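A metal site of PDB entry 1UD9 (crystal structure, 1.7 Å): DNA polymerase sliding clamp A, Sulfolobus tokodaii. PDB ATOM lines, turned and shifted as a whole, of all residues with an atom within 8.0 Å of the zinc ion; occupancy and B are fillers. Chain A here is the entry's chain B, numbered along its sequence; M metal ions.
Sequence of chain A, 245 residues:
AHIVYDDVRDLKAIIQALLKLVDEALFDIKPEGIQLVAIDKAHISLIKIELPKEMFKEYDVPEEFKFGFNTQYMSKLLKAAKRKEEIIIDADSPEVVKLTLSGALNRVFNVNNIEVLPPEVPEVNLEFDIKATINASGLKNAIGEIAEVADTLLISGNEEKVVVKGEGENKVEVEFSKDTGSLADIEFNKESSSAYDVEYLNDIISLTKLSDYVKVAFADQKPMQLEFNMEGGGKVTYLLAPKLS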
ATOM      1  N   ALA A 150      -8.301  10.473 -26.908  1.00  0.00           N
ATOM      2  CA  ALA A 150      -8.949   9.244 -27.367  1.00  0.00           C
ATOM      3  C   ALA A 150      -8.433   8.024 -26.585  1.00  0.00           C
ATOM      4  O   ALA A 150      -7.381   8.132 -25.963  1.00  0.00           O
ATOM      5  CB  ALA A 150      -8.662   9.085 -28.872  1.00  0.00           C
ATOM      6  N   ASP A 151      -9.152   6.899 -26.588  1.00  0.00           N
ATOM      7  CA  ASP A 151      -8.686   5.713 -25.879  1.00  0.00           C
ATOM      8  C   ASP A 151      -7.956   4.832 -26.870  1.00  0.00           C
ATOM      9  O   ASP A 151      -7.322   3.876 -26.476  1.00  0.00           O
ATOM     10  CB  ASP A 151      -9.810   4.824 -25.275  1.00  0.00           C
ATOM     11  CG  ASP A 151      -9.274   3.456 -24.642  1.00  0.00           C
ATOM     12  OD1 ASP A 151      -9.825   2.379 -24.965  1.00  0.00           O
ATOM     13  OD2 ASP A 151      -8.299   3.440 -23.792  1.00  0.00           O
ATOM     14  N   THR A 152      -8.095   5.173 -28.148  1.00  0.00           N
ATOM     15  CA  THR A 152      -7.538   4.338 -29.216  1.00  0.00           C
ATOM     16  C   THR A 152      -6.704   5.028 -30.214  1.00  0.00           C
ATOM     17  O   THR A 152      -6.962   6.191 -30.650  1.00  0.00           O
ATOM     18  CB  THR A 152      -8.637   3.660 -29.948  1.00  0.00           C
ATOM     19  OG1 THR A 152      -9.359   2.918 -28.998  1.00  0.00           O
ATOM     20  CG2 THR A 152      -8.097   2.707 -31.053  1.00  0.00           C
ATOM     21  N   TYR A 196      -4.915   0.012 -31.618  1.00  0.00           N
ATOM     22  CA  TYR A 196      -4.344  -0.387 -30.328  1.00  0.00           C
ATOM     23  C   TYR A 196      -4.854   0.536 -29.180  1.00  0.00           C
ATOM     24  O   TYR A 196      -5.220   1.660 -29.401  1.00  0.00           O
ATOM     25  CB  TYR A 196      -2.810  -0.280 -30.417  1.00  0.00           C
ATOM     26  CG  TYR A 196      -2.180  -1.079 -31.534  1.00  0.00           C
ATOM     27  CD1 TYR A 196      -1.970  -0.486 -32.789  1.00  0.00           C
ATOM     28  CD2 TYR A 196      -1.971  -2.468 -31.426  1.00  0.00           C
ATOM     29  CE1 TYR A 196      -1.609  -1.281 -33.886  1.00  0.00           C
ATOM     30  CE2 TYR A 196      -1.602  -3.261 -32.494  1.00  0.00           C
ATOM     31  CZ  TYR A 196      -1.428  -2.633 -33.756  1.00  0.00           C
ATOM     32  OH  TYR A 196      -1.087  -3.416 -34.817  1.00  0.00           O
ATOM     33  N   ASP A 197      -4.783   0.061 -27.920  1.00  0.00           N
ATOM     34  CA  ASP A 197      -5.209   0.848 -26.755  1.00  0.00           C
ATOM     35  C   ASP A 197      -4.076   1.811 -26.479  1.00  0.00           C
ATOM     36  O   ASP A 197      -2.979   1.366 -26.115  1.00  0.00           O
ATOM     37  CB  ASP A 197      -5.350  -0.080 -25.541  1.00  0.00           C
ATOM     38  CG  ASP A 197      -5.811   0.656 -24.310  1.00  0.00           C
ATOM     39  OD1 ASP A 197      -5.432   1.837 -24.068  1.00  0.00           O
ATOM     40  OD2 ASP A 197      -6.520   0.015 -23.564  1.00  0.00           O
ATOM     41  N   VAL A 198      -4.318   3.098 -26.621  1.00  0.00           N
ATOM     42  CA  VAL A 198      -3.300   4.085 -26.509  1.00  0.00           C
ATOM     43  C   VAL A 198      -2.825   4.253 -25.069  1.00  0.00           C
ATOM     44  O   VAL A 198      -1.698   4.730 -24.876  1.00  0.00           O
ATOM     45  CB  VAL A 198      -3.743   5.433 -27.117  1.00  0.00           C
ATOM     46  CG1 VAL A 198      -4.740   6.187 -26.203  1.00  0.00           C
ATOM     47  CG2 VAL A 198      -2.494   6.282 -27.454  1.00  0.00           C
ATOM     48  N   GLU A 199      -3.638   3.818 -24.113  1.00  0.00           N
ATOM     49  CA  GLU A 199      -3.245   3.900 -22.681  1.00  0.00           C
ATOM     50  C   GLU A 199      -2.004   3.027 -22.479  1.00  0.00           C
ATOM     51  O   GLU A 199      -1.101   3.400 -21.716  1.00  0.00           O
ATOM     52  CB  GLU A 199      -4.264   3.272 -21.696  1.00  0.00           C
ATOM     53  CG  GLU A 199      -5.738   3.601 -21.774  1.00  0.00           C
ATOM     54  CD  GLU A 199      -6.588   2.727 -20.814  1.00  0.00           C
ATOM     55  OE1 GLU A 199      -6.691   1.473 -21.016  1.00  0.00           O
ATOM     56  OE2 GLU A 199      -7.151   3.302 -19.845  1.00  0.00           O
ATOM     57  N   TYR A 200      -1.984   1.860 -23.106  1.00  0.00           N
ATOM     58  CA  TYR A 200      -0.820   0.991 -22.930  1.00  0.00           C
ATOM     59  C   TYR A 200       0.413   1.616 -23.545  1.00  0.00           C
ATOM     60  O   TYR A 200       1.521   1.591 -22.964  1.00  0.00           O
ATOM     61  CB  TYR A 200      -1.037  -0.399 -23.544  1.00  0.00           C
ATOM     62  CG  TYR A 200      -1.972  -1.255 -22.763  1.00  0.00           C
ATOM     63  CD1 TYR A 200      -3.301  -0.856 -22.541  1.00  0.00           C
ATOM     64  CD2 TYR A 200      -1.529  -2.470 -22.226  1.00  0.00           C
ATOM     65  CE1 TYR A 200      -4.148  -1.664 -21.796  1.00  0.00           C
ATOM     66  CE2 TYR A 200      -2.371  -3.254 -21.478  1.00  0.00           C
ATOM     67  CZ  TYR A 200      -3.666  -2.856 -21.278  1.00  0.00           C
ATOM     68  OH  TYR A 200      -4.506  -3.750 -20.677  1.00  0.00           O
ATOM     69  N   LYS A 243      -6.487  -4.269 -31.198  1.00  0.00           N
ATOM     70  CA  LYS A 243      -7.930  -4.200 -31.036  1.00  0.00           C
ATOM     71  C   LYS A 243      -8.461  -4.449 -32.470  1.00  0.00           C
ATOM     72  O   LYS A 243      -7.690  -4.538 -33.422  1.00  0.00           O
ATOM     73  CB  LYS A 243      -8.398  -2.836 -30.603  1.00  0.00           C
ATOM     74  CG  LYS A 243      -7.965  -2.516 -29.155  1.00  0.00           C
ATOM     75  CD  LYS A 243      -8.465  -3.635 -28.198  1.00  0.00           C
ATOM     76  CE  LYS A 243      -8.437  -3.244 -26.684  1.00  0.00           C
ATOM     77  NZ  LYS A 243      -9.394  -2.045 -26.387  1.00  0.00           N
HETATM   78 ZN    ZN M   1      -8.126   1.176 -23.054  1.00  0.00          ZN
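Three residues have an atom within 4 Å of the zinc ion: Asp 151, Asp 197 and Glu 199.
The zinc ion is bound by the side-chain carboxylate (OD2) of Asp 197 (2.0 Å), the side-chain carboxylate (OD2) of Asp 151 (2.4 Å) and the side-chain carboxylate (OE1) of Glu 199 (2.5 Å).
The zinc ion has three donor atoms within binding distance.
Slightly farther from the zinc ion lies OD1 of Asp 151 (2.8 Å).
O of Asp 151 lies within hydrogen-bond range of N of Val 198.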
